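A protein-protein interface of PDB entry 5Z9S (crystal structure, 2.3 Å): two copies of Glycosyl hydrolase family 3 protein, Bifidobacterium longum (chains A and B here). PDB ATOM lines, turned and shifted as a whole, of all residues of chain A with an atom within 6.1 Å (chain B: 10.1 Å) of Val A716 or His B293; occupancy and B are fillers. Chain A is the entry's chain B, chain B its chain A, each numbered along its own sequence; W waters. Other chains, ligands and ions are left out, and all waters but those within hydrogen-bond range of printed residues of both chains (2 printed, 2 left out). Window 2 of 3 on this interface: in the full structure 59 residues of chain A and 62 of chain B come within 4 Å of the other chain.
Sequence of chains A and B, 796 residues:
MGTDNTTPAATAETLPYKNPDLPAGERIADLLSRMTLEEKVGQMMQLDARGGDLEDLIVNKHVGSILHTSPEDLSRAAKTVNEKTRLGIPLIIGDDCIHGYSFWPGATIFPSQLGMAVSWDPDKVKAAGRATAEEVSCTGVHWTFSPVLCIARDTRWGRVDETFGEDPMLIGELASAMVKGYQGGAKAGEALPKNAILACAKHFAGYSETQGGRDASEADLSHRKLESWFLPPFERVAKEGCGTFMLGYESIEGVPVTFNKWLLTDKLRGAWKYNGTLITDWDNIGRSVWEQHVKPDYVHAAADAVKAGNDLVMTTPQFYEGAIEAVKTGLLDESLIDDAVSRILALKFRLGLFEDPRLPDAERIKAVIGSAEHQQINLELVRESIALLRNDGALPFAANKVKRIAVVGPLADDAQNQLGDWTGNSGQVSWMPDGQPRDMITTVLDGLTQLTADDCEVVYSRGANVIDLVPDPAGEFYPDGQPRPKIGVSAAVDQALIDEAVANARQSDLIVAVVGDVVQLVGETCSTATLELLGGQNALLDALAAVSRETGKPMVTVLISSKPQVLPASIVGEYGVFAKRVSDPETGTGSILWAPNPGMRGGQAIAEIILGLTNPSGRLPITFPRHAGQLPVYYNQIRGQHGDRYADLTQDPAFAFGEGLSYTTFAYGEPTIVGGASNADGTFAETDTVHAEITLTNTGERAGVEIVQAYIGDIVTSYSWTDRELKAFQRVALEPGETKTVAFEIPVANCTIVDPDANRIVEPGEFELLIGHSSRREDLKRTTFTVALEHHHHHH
The backbone carbonyl oxygen of Gly B254 lies within hydrogen-bond range of the backbone NH of Ser A720, 3.0 Å away. The side-chain hydroxyl (OG) of Ser B251 lies within hydrogen-bond range of the side-chain hydroxyl (OG) of Ser A720, 2.8 Å away. The side-chain carboxylate (OE2) of Glu B218 is in hydrogen-bond range of the side-chain hydroxyl (OG) of Ser A720 (2.7 Å). O of Thr A717 sits close to O of Val B294 (3.1 Å). The backbone carbonyl oxygen (O) of His B293 sits at hydrogen-bond distance from the backbone NH (N) of Thr A717, at 3.2 Å.
O of Ile A715 touches CD2 of His B293, 3.6 Å away. His B293 touches Val A716. Val B294 touches Ser A718 (CG1 to O, 3.6 Å). Tyr A719 touches Gly B254 (CA to O, 3.3 Å). Val B294 touches Ser A720.
N of Ile A715 lies within hydrogen-bond range of O of Glu A766, at 3.1 Å. OG1 of Thr A717 sits at hydrogen-bond distance from O of Tyr A719 (2.7 Å). OE2 of Glu B218 is in hydrogen-bond range of OG of Ser B251 (3.4 Å). The backbone carbonyl oxygen (O) of Ser B288 sits at hydrogen-bond distance from the backbone NH (N) of Val B294 (2.9 Å). OE2 of Glu A763 is in hydrogen-bond range of OG of Ser A718, 2.7 Å away. The backbone NH (N) of Gly B254 is in hydrogen-bond range of the side-chain carboxylate (OE1) of Glu B218, at 3.0 Å.
Water W2 lies within hydrogen-bond range of the backbone carbonyl oxygen (O) of Ser A720 (2.6 Å) and the side-chain carboxylate (OE1) of Glu B218 (2.8 Å). Water W1 lies within hydrogen-bond range of the backbone carbonyl oxygen of Gln B292 (2.7 Å), the side-chain hydroxyl of Thr A717 (2.9 Å), the guanidinium group of Arg A639 (3.3 Å) and the backbone carbonyl oxygen of His B293 (3.4 Å).
No position is printed for both chains.
Val A716 touches just one residue of chain B: His B293. Of chain A, only Ile A715, Val A716 and Thr A717 come within 4 Å of His B293. Ile A715 touches one residue of chain B. Thr A717 touches just these residues of chain B: His B293 (3.2 Å) and Val B294 (3.1 Å). Of the printed residues of chain B, Ser A720 touches Glu B218, Ser B251, Gly B254 and Val B294. Of the printed residues of chain A, Val B294 touches Thr A717, Ser A718 and Ser A720. Of the printed residues of chain A, Glu B218 touches Ser A720. Of the printed residues of chain B, Tyr A719 touches Gly B254. Of the printed residues of chain B, Ser A718 touches Val B294 (3.6 Å). The nearest residue of chain B that does not touch Val A716 is Pro B296 (4.2 Å). The nearest printed residue of chain A that does not touch Glu B218 is Arg A639 (4.6 Å).
Printed residues of chain A that touch a printed residue of chain B: Ile A715, Val A716, Thr A717, Ser A718, Tyr A719 and Ser A720. Hydrophobic or aromatic side chains of chain A that line the printed part of chain B: Val A716 and Tyr A719. Printed residues of chain B that touch a printed residue of chain A: Glu B218, Ser B251, Gly B254, His B293 and Val B294. Hydrophobic or aromatic side chains of chain B that line the printed part of chain A: His B293 and Val B294. Among the printed residues, 10 pairs touch across the chains.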
ATOM      1  N   ARG A 639     -23.805  25.026  -8.713  1.00  0.00           N
ATOM      2  CA  ARG A 639     -23.305  23.724  -9.137  1.00  0.00           C
ATOM      3  C   ARG A 639     -24.231  23.087 -10.168  1.00  0.00           C
ATOM      4  O   ARG A 639     -25.436  23.348 -10.200  1.00  0.00           O
ATOM      5  CB  ARG A 639     -23.174  22.773  -7.949  1.00  0.00           C
ATOM      6  CG  ARG A 639     -22.339  23.270  -6.795  1.00  0.00           C
ATOM      7  CD  ARG A 639     -22.939  22.779  -5.493  1.00  0.00           C
ATOM      8  NE  ARG A 639     -21.957  22.696  -4.424  1.00  0.00           N
ATOM      9  CZ  ARG A 639     -22.265  22.596  -3.136  1.00  0.00           C
ATOM     10  NH1 ARG A 639     -23.535  22.582  -2.756  1.00  0.00           N
ATOM     11  NH2 ARG A 639     -21.304  22.522  -2.230  1.00  0.00           N
ATOM     12  N   ASP A 714     -21.761  24.913   1.757  1.00  0.00           N
ATOM     13  CA  ASP A 714     -22.641  23.832   2.182  1.00  0.00           C
ATOM     14  C   ASP A 714     -22.409  22.653   1.241  1.00  0.00           C
ATOM     15  O   ASP A 714     -22.744  22.724   0.055  1.00  0.00           O
ATOM     16  CB  ASP A 714     -24.097  24.291   2.169  1.00  0.00           C
ATOM     17  CG  ASP A 714     -25.022  23.347   2.913  1.00  0.00           C
ATOM     18  OD1 ASP A 714     -24.661  22.171   3.125  1.00  0.00           O
ATOM     19  OD2 ASP A 714     -26.132  23.784   3.276  1.00  0.00           O
ATOM     20  N   ILE A 715     -21.836  21.571   1.773  1.00  0.00           N
ATOM     21  CA  ILE A 715     -21.342  20.487   0.925  1.00  0.00           C
ATOM     22  C   ILE A 715     -22.491  19.827   0.171  1.00  0.00           C
ATOM     23  O   ILE A 715     -22.407  19.592  -1.040  1.00  0.00           O
ATOM     24  CB  ILE A 715     -20.557  19.466   1.766  1.00  0.00           C
ATOM     25  CG1 ILE A 715     -19.313  20.122   2.362  1.00  0.00           C
ATOM     26  CG2 ILE A 715     -20.161  18.269   0.916  1.00  0.00           C
ATOM     27  CD1 ILE A 715     -18.374  20.688   1.321  1.00  0.00           C
ATOM     28  N   VAL A 716     -23.571  19.504   0.875  1.00  0.00           N
ATOM     29  CA  VAL A 716     -24.768  18.928   0.274  1.00  0.00           C
ATOM     30  C   VAL A 716     -25.950  19.821   0.622  1.00  0.00           C
ATOM     31  O   VAL A 716     -26.125  20.203   1.784  1.00  0.00           O
ATOM     32  CB  VAL A 716     -25.014  17.484   0.752  1.00  0.00           C
ATOM     33  CG1 VAL A 716     -26.151  16.855  -0.038  1.00  0.00           C
ATOM     34  CG2 VAL A 716     -23.750  16.653   0.611  1.00  0.00           C
ATOM     35  N   THR A 717     -26.758  20.151  -0.383  1.00  0.00           N
ATOM     36  CA  THR A 717     -27.928  20.998  -0.205  1.00  0.00           C
ATOM     37  C   THR A 717     -29.132  20.326  -0.848  1.00  0.00           C
ATOM     38  O   THR A 717     -29.017  19.734  -1.923  1.00  0.00           O
ATOM     39  CB  THR A 717     -27.726  22.391  -0.825  1.00  0.00           C
ATOM     40  OG1 THR A 717     -27.390  22.264  -2.213  1.00  0.00           O
ATOM     41  CG2 THR A 717     -26.615  23.132  -0.118  1.00  0.00           C
ATOM     42  N   SER A 718     -30.289  20.432  -0.188  1.00  0.00           N
ATOM     43  CA  SER A 718     -31.509  19.837  -0.724  1.00  0.00           C
ATOM     44  C   SER A 718     -31.930  20.475  -2.038  1.00  0.00           C
ATOM     45  O   SER A 718     -32.651  19.847  -2.820  1.00  0.00           O
ATOM     46  CB  SER A 718     -32.648  19.954   0.287  1.00  0.00           C
ATOM     47  OG  SER A 718     -32.349  19.248   1.474  1.00  0.00           O
ATOM     48  N   TYR A 719     -31.521  21.713  -2.283  1.00  0.00           N
ATOM     49  CA  TYR A 719     -31.804  22.413  -3.525  1.00  0.00           C
ATOM     50  C   TYR A 719     -30.499  22.992  -4.044  1.00  0.00           C
ATOM     51  O   TYR A 719     -29.644  23.405  -3.255  1.00  0.00           O
ATOM     52  CB  TYR A 719     -32.856  23.503  -3.304  1.00  0.00           C
ATOM     53  CG  TYR A 719     -34.002  23.012  -2.449  1.00  0.00           C
ATOM     54  CD1 TYR A 719     -34.988  22.192  -2.983  1.00  0.00           C
ATOM     55  CD2 TYR A 719     -34.078  23.336  -1.102  1.00  0.00           C
ATOM     56  CE1 TYR A 719     -36.029  21.723  -2.203  1.00  0.00           C
ATOM     57  CE2 TYR A 719     -35.116  22.871  -0.313  1.00  0.00           C
ATOM     58  CZ  TYR A 719     -36.089  22.064  -0.869  1.00  0.00           C
ATOM     59  OH  TYR A 719     -37.124  21.605  -0.088  1.00  0.00           O
ATOM     60  N   SER A 720     -30.343  23.004  -5.367  1.00  0.00           N
ATOM     61  CA  SER A 720     -29.066  23.375  -5.963  1.00  0.00           C
ATOM     62  C   SER A 720     -28.647  24.767  -5.509  1.00  0.00           C
ATOM     63  O   SER A 720     -29.460  25.693  -5.435  1.00  0.00           O
ATOM     64  CB  SER A 720     -29.142  23.307  -7.491  1.00  0.00           C
ATOM     65  OG  SER A 720     -29.985  24.312  -8.018  1.00  0.00           O
ATOM     66  N   GLU A 763     -29.587  24.358   6.957  1.00  0.00           N
ATOM     67  CA  GLU A 763     -29.808  22.947   6.717  1.00  0.00           C
ATOM     68  C   GLU A 763     -28.722  22.133   7.396  1.00  0.00           C
ATOM     69  O   GLU A 763     -27.533  22.383   7.159  1.00  0.00           O
ATOM     70  CB  GLU A 763     -29.825  22.651   5.218  1.00  0.00           C
ATOM     71  CG  GLU A 763     -30.737  21.513   4.840  1.00  0.00           C
ATOM     72  CD  GLU A 763     -30.939  21.412   3.349  1.00  0.00           C
ATOM     73  OE1 GLU A 763     -29.938  21.234   2.622  1.00  0.00           O
ATOM     74  OE2 GLU A 763     -32.099  21.539   2.903  1.00  0.00           O
ATOM     75  N   PRO A 764     -29.080  21.170   8.242  1.00  0.00           N
ATOM     76  CA  PRO A 764     -28.056  20.356   8.905  1.00  0.00           C
ATOM     77  C   PRO A 764     -27.233  19.571   7.896  1.00  0.00           C
ATOM     78  O   PRO A 764     -27.722  19.162   6.841  1.00  0.00           O
ATOM     79  CB  PRO A 764     -28.871  19.427   9.814  1.00  0.00           C
ATOM     80  CG  PRO A 764     -30.243  19.417   9.218  1.00  0.00           C
ATOM     81  CD  PRO A 764     -30.441  20.787   8.649  1.00  0.00           C
ATOM     82  N   GLY A 765     -25.970  19.374   8.230  1.00  0.00           N
ATOM     83  CA  GLY A 765     -25.055  18.665   7.368  1.00  0.00           C
ATOM     84  C   GLY A 765     -23.656  19.232   7.505  1.00  0.00           C
ATOM     85  O   GLY A 765     -23.360  19.971   8.440  1.00  0.00           O
ATOM     86  N   GLU A 766     -22.816  18.882   6.539  1.00  0.00           N
ATOM     87  CA  GLU A 766     -21.406  19.239   6.563  1.00  0.00           C
ATOM     88  C   GLU A 766     -21.170  20.560   5.841  1.00  0.00           C
ATOM     89  O   GLU A 766     -21.744  20.818   4.781  1.00  0.00           O
ATOM     90  CB  GLU A 766     -20.570  18.135   5.913  1.00  0.00           C
ATOM     91  CG  GLU A 766     -19.086  18.209   6.220  1.00  0.00           C
ATOM     92  CD  GLU A 766     -18.290  17.184   5.440  1.00  0.00           C
ATOM     93  OE1 GLU A 766     -18.860  16.571   4.512  1.00  0.00           O
ATOM     94  OE2 GLU A 766     -17.099  16.984   5.755  1.00  0.00           O
ATOM     95  N   ALA B 216     -25.503  22.101 -18.587  1.00  0.00           N
ATOM     96  CA  ALA B 216     -26.514  21.842 -17.569  1.00  0.00           C
ATOM     97  C   ALA B 216     -26.308  22.731 -16.353  1.00  0.00           C
ATOM     98  O   ALA B 216     -26.474  22.302 -15.212  1.00  0.00           O
ATOM     99  CB  ALA B 216     -26.530  20.371 -17.168  1.00  0.00           C
ATOM    100  N   GLU B 218     -27.421  26.149 -14.041  1.00  0.00           N
ATOM    101  CA  GLU B 218     -28.695  26.419 -13.389  1.00  0.00           C
ATOM    102  C   GLU B 218     -29.678  27.085 -14.346  1.00  0.00           C
ATOM    103  O   GLU B 218     -29.312  27.962 -15.134  1.00  0.00           O
ATOM    104  CB  GLU B 218     -28.473  27.303 -12.163  1.00  0.00           C
ATOM    105  CG  GLU B 218     -29.736  27.627 -11.381  1.00  0.00           C
ATOM    106  CD  GLU B 218     -30.219  26.473 -10.522  1.00  0.00           C
ATOM    107  OE1 GLU B 218     -31.275  26.624  -9.877  1.00  0.00           O
ATOM    108  OE2 GLU B 218     -29.551  25.420 -10.483  1.00  0.00           O
ATOM    109  N   SER B 251     -31.124  21.656 -13.227  1.00  0.00           N
ATOM    110  CA  SER B 251     -31.883  22.018 -12.041  1.00  0.00           C
ATOM    111  C   SER B 251     -32.616  23.327 -12.308  1.00  0.00           C
ATOM    112  O   SER B 251     -31.996  24.322 -12.697  1.00  0.00           O
ATOM    113  CB  SER B 251     -30.955  22.144 -10.834  1.00  0.00           C
ATOM    114  OG  SER B 251     -31.608  22.766  -9.744  1.00  0.00           O
ATOM    115  N   GLY B 254     -33.492  25.369  -8.341  1.00  0.00           N
ATOM    116  CA  GLY B 254     -33.041  24.513  -7.267  1.00  0.00           C
ATOM    117  C   GLY B 254     -33.508  23.074  -7.337  1.00  0.00           C
ATOM    118  O   GLY B 254     -33.051  22.257  -6.529  1.00  0.00           O
ATOM    119  N   PRO B 256     -33.915  19.741  -9.824  1.00  0.00           N
ATOM    120  CA  PRO B 256     -33.783  19.047 -11.110  1.00  0.00           C
ATOM    121  C   PRO B 256     -35.124  18.503 -11.584  1.00  0.00           C
ATOM    122  O   PRO B 256     -35.988  18.141 -10.784  1.00  0.00           O
ATOM    123  CB  PRO B 256     -32.795  17.916 -10.804  1.00  0.00           C
ATOM    124  CG  PRO B 256     -32.029  18.394  -9.621  1.00  0.00           C
ATOM    125  CD  PRO B 256     -33.003  19.195  -8.805  1.00  0.00           C
ATOM    126  N   PHE B 259     -37.025  15.391 -10.247  1.00  0.00           N
ATOM    127  CA  PHE B 259     -37.791  15.468  -9.010  1.00  0.00           C
ATOM    128  C   PHE B 259     -38.750  16.651  -8.993  1.00  0.00           C
ATOM    129  O   PHE B 259     -39.270  16.995  -7.927  1.00  0.00           O
ATOM    130  CB  PHE B 259     -36.848  15.545  -7.807  1.00  0.00           C
ATOM    131  CG  PHE B 259     -35.615  14.700  -7.949  1.00  0.00           C
ATOM    132  CD1 PHE B 259     -35.654  13.339  -7.687  1.00  0.00           C
ATOM    133  CD2 PHE B 259     -34.416  15.266  -8.351  1.00  0.00           C
ATOM    134  CE1 PHE B 259     -34.521  12.560  -7.819  1.00  0.00           C
ATOM    135  CE2 PHE B 259     -33.279  14.492  -8.487  1.00  0.00           C
ATOM    136  CZ  PHE B 259     -33.332  13.136  -8.219  1.00  0.00           C
ATOM    137  N   ASN B 284     -29.519  11.109 -14.906  1.00  0.00           N
ATOM    138  CA  ASN B 284     -30.060  12.215 -14.122  1.00  0.00           C
ATOM    139  C   ASN B 284     -29.946  11.943 -12.626  1.00  0.00           C
ATOM    140  O   ASN B 284     -29.550  12.825 -11.851  1.00  0.00           O
ATOM    141  CB  ASN B 284     -31.520  12.459 -14.504  1.00  0.00           C
ATOM    142  CG  ASN B 284     -31.669  13.234 -15.793  1.00  0.00           C
ATOM    143  OD1 ASN B 284     -30.692  13.508 -16.485  1.00  0.00           O
ATOM    144  ND2 ASN B 284     -32.903  13.584 -16.129  1.00  0.00           N
ATOM    145  N   ILE B 285     -30.288  10.725 -12.204  1.00  0.00           N
ATOM    146  CA  ILE B 285     -30.322  10.402 -10.780  1.00  0.00           C
ATOM    147  C   ILE B 285     -28.922  10.456 -10.180  1.00  0.00           C
ATOM    148  O   ILE B 285     -28.713  11.019  -9.099  1.00  0.00           O
ATOM    149  CB  ILE B 285     -30.980   9.030 -10.566  1.00  0.00           C
ATOM    150  CG1 ILE B 285     -32.458   9.097 -10.952  1.00  0.00           C
ATOM    151  CG2 ILE B 285     -30.817   8.580  -9.125  1.00  0.00           C
ATOM    152  CD1 ILE B 285     -33.149   7.759 -10.930  1.00  0.00           C
ATOM    153  N   GLY B 286     -27.942   9.868 -10.869  1.00  0.00           N
ATOM    154  CA  GLY B 286     -26.573   9.937 -10.384  1.00  0.00           C
ATOM    155  C   GLY B 286     -26.040  11.354 -10.359  1.00  0.00           C
ATOM    156  O   GLY B 286     -25.410  11.775  -9.382  1.00  0.00           O
ATOM    157  N   ARG B 287     -26.288  12.112 -11.431  1.00  0.00           N
ATOM    158  CA  ARG B 287     -25.857  13.504 -11.472  1.00  0.00           C
ATOM    159  C   ARG B 287     -26.445  14.306 -10.321  1.00  0.00           C
ATOM    160  O   ARG B 287     -25.787  15.216  -9.806  1.00  0.00           O
ATOM    161  CB  ARG B 287     -26.249  14.144 -12.801  1.00  0.00           C
ATOM    162  CG  ARG B 287     -25.460  13.656 -13.997  1.00  0.00           C
ATOM    163  CD  ARG B 287     -26.007  14.279 -15.267  1.00  0.00           C
ATOM    164  NE  ARG B 287     -25.636  13.536 -16.464  1.00  0.00           N
ATOM    165  CZ  ARG B 287     -24.508  13.721 -17.137  1.00  0.00           C
ATOM    166  NH1 ARG B 287     -23.628  14.621 -16.721  1.00  0.00           N
ATOM    167  NH2 ARG B 287     -24.257  13.004 -18.222  1.00  0.00           N
ATOM    168  N   SER B 288     -27.675  13.987  -9.903  1.00  0.00           N
ATOM    169  CA  SER B 288     -28.238  14.651  -8.732  1.00  0.00           C
ATOM    170  C   SER B 288     -27.383  14.433  -7.491  1.00  0.00           C
ATOM    171  O   SER B 288     -27.451  15.237  -6.555  1.00  0.00           O
ATOM    172  CB  SER B 288     -29.667  14.168  -8.468  1.00  0.00           C
ATOM    173  OG  SER B 288     -29.693  12.809  -8.065  1.00  0.00           O
ATOM    174  N   VAL B 289     -26.574  13.375  -7.471  1.00  0.00           N
ATOM    175  CA  VAL B 289     -25.723  13.064  -6.330  1.00  0.00           C
ATOM    176  C   VAL B 289     -24.332  13.655  -6.522  1.00  0.00           C
ATOM    177  O   VAL B 289     -23.897  14.502  -5.734  1.00  0.00           O
ATOM    178  CB  VAL B 289     -25.643  11.545  -6.099  1.00  0.00           C
ATOM    179  CG1 VAL B 289     -24.674  11.232  -4.968  1.00  0.00           C
ATOM    180  CG2 VAL B 289     -27.024  10.984  -5.803  1.00  0.00           C
ATOM    181  N   TRP B 290     -23.615  13.215  -7.561  1.00  0.00           N
ATOM    182  CA  TRP B 290     -22.204  13.571  -7.665  1.00  0.00           C
ATOM    183  C   TRP B 290     -21.952  14.880  -8.401  1.00  0.00           C
ATOM    184  O   TRP B 290     -20.895  15.488  -8.197  1.00  0.00           O
ATOM    185  CB  TRP B 290     -21.404  12.445  -8.341  1.00  0.00           C
ATOM    186  CG  TRP B 290     -21.830  12.083  -9.739  1.00  0.00           C
ATOM    187  CD1 TRP B 290     -22.660  11.062 -10.103  1.00  0.00           C
ATOM    188  CD2 TRP B 290     -21.422  12.720 -10.959  1.00  0.00           C
ATOM    189  NE1 TRP B 290     -22.808  11.033 -11.470  1.00  0.00           N
ATOM    190  CE2 TRP B 290     -22.058  12.040 -12.019  1.00  0.00           C
ATOM    191  CE3 TRP B 290     -20.587  13.802 -11.259  1.00  0.00           C
ATOM    192  CZ2 TRP B 290     -21.887  12.406 -13.353  1.00  0.00           C
ATOM    193  CZ3 TRP B 290     -20.418  14.164 -12.586  1.00  0.00           C
ATOM    194  CH2 TRP B 290     -21.066  13.467 -13.616  1.00  0.00           C
ATOM    195  N   GLU B 291     -22.886  15.351  -9.220  1.00  0.00           N
ATOM    196  CA  GLU B 291     -22.659  16.553 -10.011  1.00  0.00           C
ATOM    197  C   GLU B 291     -23.395  17.776  -9.484  1.00  0.00           C
ATOM    198  O   GLU B 291     -22.811  18.860  -9.431  1.00  0.00           O
ATOM    199  CB  GLU B 291     -23.057  16.301 -11.471  1.00  0.00           C
ATOM    200  CG  GLU B 291     -22.378  17.217 -12.480  1.00  0.00           C
ATOM    201  CD  GLU B 291     -22.458  16.679 -13.904  1.00  0.00           C
ATOM    202  OE1 GLU B 291     -23.509  16.109 -14.256  1.00  0.00           O
ATOM    203  OE2 GLU B 291     -21.479  16.829 -14.667  1.00  0.00           O
ATOM    204  N   GLN B 292     -24.660  17.637  -9.089  1.00  0.00           N
ATOM    205  CA  GLN B 292     -25.439  18.752  -8.566  1.00  0.00           C
ATOM    206  C   GLN B 292     -25.383  18.870  -7.047  1.00  0.00           C
ATOM    207  O   GLN B 292     -25.792  19.906  -6.510  1.00  0.00           O
ATOM    208  CB  GLN B 292     -26.902  18.623  -9.011  1.00  0.00           C
ATOM    209  CG  GLN B 292     -27.143  18.987 -10.470  1.00  0.00           C
ATOM    210  CD  GLN B 292     -28.351  18.283 -11.063  1.00  0.00           C
ATOM    211  OE1 GLN B 292     -28.761  17.227 -10.583  1.00  0.00           O
ATOM    212  NE2 GLN B 292     -28.918  18.859 -12.115  1.00  0.00           N
ATOM    213  N   HIS B 293     -24.886  17.846  -6.348  1.00  0.00           N
ATOM    214  CA  HIS B 293     -24.819  17.845  -4.884  1.00  0.00           C
ATOM    215  C   HIS B 293     -26.181  18.172  -4.274  1.00  0.00           C
ATOM    216  O   HIS B 293     -26.292  18.943  -3.319  1.00  0.00           O
ATOM    217  CB  HIS B 293     -23.741  18.806  -4.369  1.00  0.00           C
ATOM    218  CG  HIS B 293     -22.350  18.441  -4.786  1.00  0.00           C
ATOM    219  ND1 HIS B 293     -21.934  18.456  -6.100  1.00  0.00           N
ATOM    220  CD2 HIS B 293     -21.275  18.054  -4.057  1.00  0.00           C
ATOM    221  CE1 HIS B 293     -20.666  18.090  -6.165  1.00  0.00           C
ATOM    222  NE2 HIS B 293     -20.243  17.839  -4.939  1.00  0.00           N
ATOM    223  N   VAL B 294     -27.231  17.574  -4.837  1.00  0.00           N
ATOM    224  CA  VAL B 294     -28.601  17.829  -4.404  1.00  0.00           C
ATOM    225  C   VAL B 294     -29.105  16.664  -3.558  1.00  0.00           C
ATOM    226  O   VAL B 294     -29.856  16.863  -2.595  1.00  0.00           O
ATOM    227  CB  VAL B 294     -29.514  18.091  -5.617  1.00  0.00           C
ATOM    228  CG1 VAL B 294     -30.964  17.805  -5.283  1.00  0.00           C
ATOM    229  CG2 VAL B 294     -29.358  19.526  -6.081  1.00  0.00           C
ATOM    230  N   LYS B 295     -28.686  15.436  -3.901  1.00  0.00           N
ATOM    231  CA  LYS B 295     -29.090  14.276  -3.119  1.00  0.00           C
ATOM    232  C   LYS B 295     -27.912  13.720  -2.327  1.00  0.00           C
ATOM    233  O   LYS B 295     -26.781  13.715  -2.825  1.00  0.00           O
ATOM    234  CB  LYS B 295     -29.665  13.172  -4.015  1.00  0.00           C
ATOM    235  CG  LYS B 295     -30.893  13.594  -4.797  1.00  0.00           C
ATOM    236  CD  LYS B 295     -32.000  14.053  -3.862  1.00  0.00           C
ATOM    237  CE  LYS B 295     -33.148  14.680  -4.629  1.00  0.00           C
ATOM    238  NZ  LYS B 295     -34.249  15.098  -3.720  1.00  0.00           N
ATOM    239  N   PRO B 296     -28.145  13.237  -1.102  1.00  0.00           N
ATOM    240  CA  PRO B 296     -27.010  12.776  -0.283  1.00  0.00           C
ATOM    241  C   PRO B 296     -26.391  11.484  -0.781  1.00  0.00           C
ATOM    242  O   PRO B 296     -25.163  11.340  -0.749  1.00  0.00           O
ATOM    243  CB  PRO B 296     -27.633  12.609   1.110  1.00  0.00           C
ATOM    244  CG  PRO B 296     -29.078  12.330   0.840  1.00  0.00           C
ATOM    245  CD  PRO B 296     -29.435  13.095  -0.404  1.00  0.00           C
ATOM    246  N   ASP B 297     -27.205  10.539  -1.247  1.00  0.00           N
ATOM    247  CA  ASP B 297     -26.707   9.274  -1.765  1.00  0.00           C
ATOM    248  C   ASP B 297     -27.704   8.736  -2.782  1.00  0.00           C
ATOM    249  O   ASP B 297     -28.751   9.339  -3.033  1.00  0.00           O
ATOM    250  CB  ASP B 297     -26.452   8.278  -0.629  1.00  0.00           C
ATOM    251  CG  ASP B 297     -27.627   8.165   0.328  1.00  0.00           C
ATOM    252  OD1 ASP B 297     -28.770   7.957  -0.136  1.00  0.00           O
ATOM    253  OD2 ASP B 297     -27.404   8.285   1.551  1.00  0.00           O
ATOM    254  N   TYR B 298     -27.368   7.584  -3.368  1.00  0.00           N
ATOM    255  CA  TYR B 298     -28.202   6.991  -4.407  1.00  0.00           C
ATOM    256  C   TYR B 298     -29.487   6.384  -3.859  1.00  0.00           C
ATOM    257  O   TYR B 298     -30.440   6.199  -4.623  1.00  0.00           O
ATOM    258  CB  TYR B 298     -27.410   5.931  -5.178  1.00  0.00           C
ATOM    259  CG  TYR B 298     -26.272   6.506  -5.989  1.00  0.00           C
ATOM    260  CD1 TYR B 298     -25.015   6.691  -5.430  1.00  0.00           C
ATOM    261  CD2 TYR B 298     -26.462   6.882  -7.313  1.00  0.00           C
ATOM    262  CE1 TYR B 298     -23.975   7.227  -6.170  1.00  0.00           C
ATOM    263  CE2 TYR B 298     -25.431   7.416  -8.062  1.00  0.00           C
ATOM    264  CZ  TYR B 298     -24.190   7.588  -7.485  1.00  0.00           C
ATOM    265  OH  TYR B 298     -23.161   8.121  -8.228  1.00  0.00           O
ATOM    266  N   HIS B 300     -31.534   7.776  -1.412  1.00  0.00           N
ATOM    267  CA  HIS B 300     -32.510   8.861  -1.375  1.00  0.00           C
ATOM    268  C   HIS B 300     -32.805   9.394  -2.771  1.00  0.00           C
ATOM    269  O   HIS B 300     -33.943   9.771  -3.068  1.00  0.00           O
ATOM    270  CB  HIS B 300     -32.010   9.985  -0.468  1.00  0.00           C
ATOM    271  CG  HIS B 300     -31.968   9.616   0.980  1.00  0.00           C
ATOM    272  ND1 HIS B 300     -30.927   8.905   1.538  1.00  0.00           N
ATOM    273  CD2 HIS B 300     -32.837   9.864   1.989  1.00  0.00           C
ATOM    274  CE1 HIS B 300     -31.159   8.726   2.826  1.00  0.00           C
ATOM    275  NE2 HIS B 300     -32.310   9.300   3.125  1.00  0.00           N
ATOM    276  N   ALA B 301     -31.796   9.436  -3.643  1.00  0.00           N
ATOM    277  CA  ALA B 301     -32.025   9.891  -5.010  1.00  0.00           C
ATOM    278  C   ALA B 301     -32.983   8.958  -5.740  1.00  0.00           C
ATOM    279  O   ALA B 301     -33.929   9.408  -6.398  1.00  0.00           O
ATOM    280  CB  ALA B 301     -30.697  10.002  -5.757  1.00  0.00           C
HETATM  281  O   HOH W   1     -26.038  21.987  -4.783  1.00  0.00           O
HETATM  282  O   HOH W   2     -30.399  27.268  -7.280  1.00  0.00           O
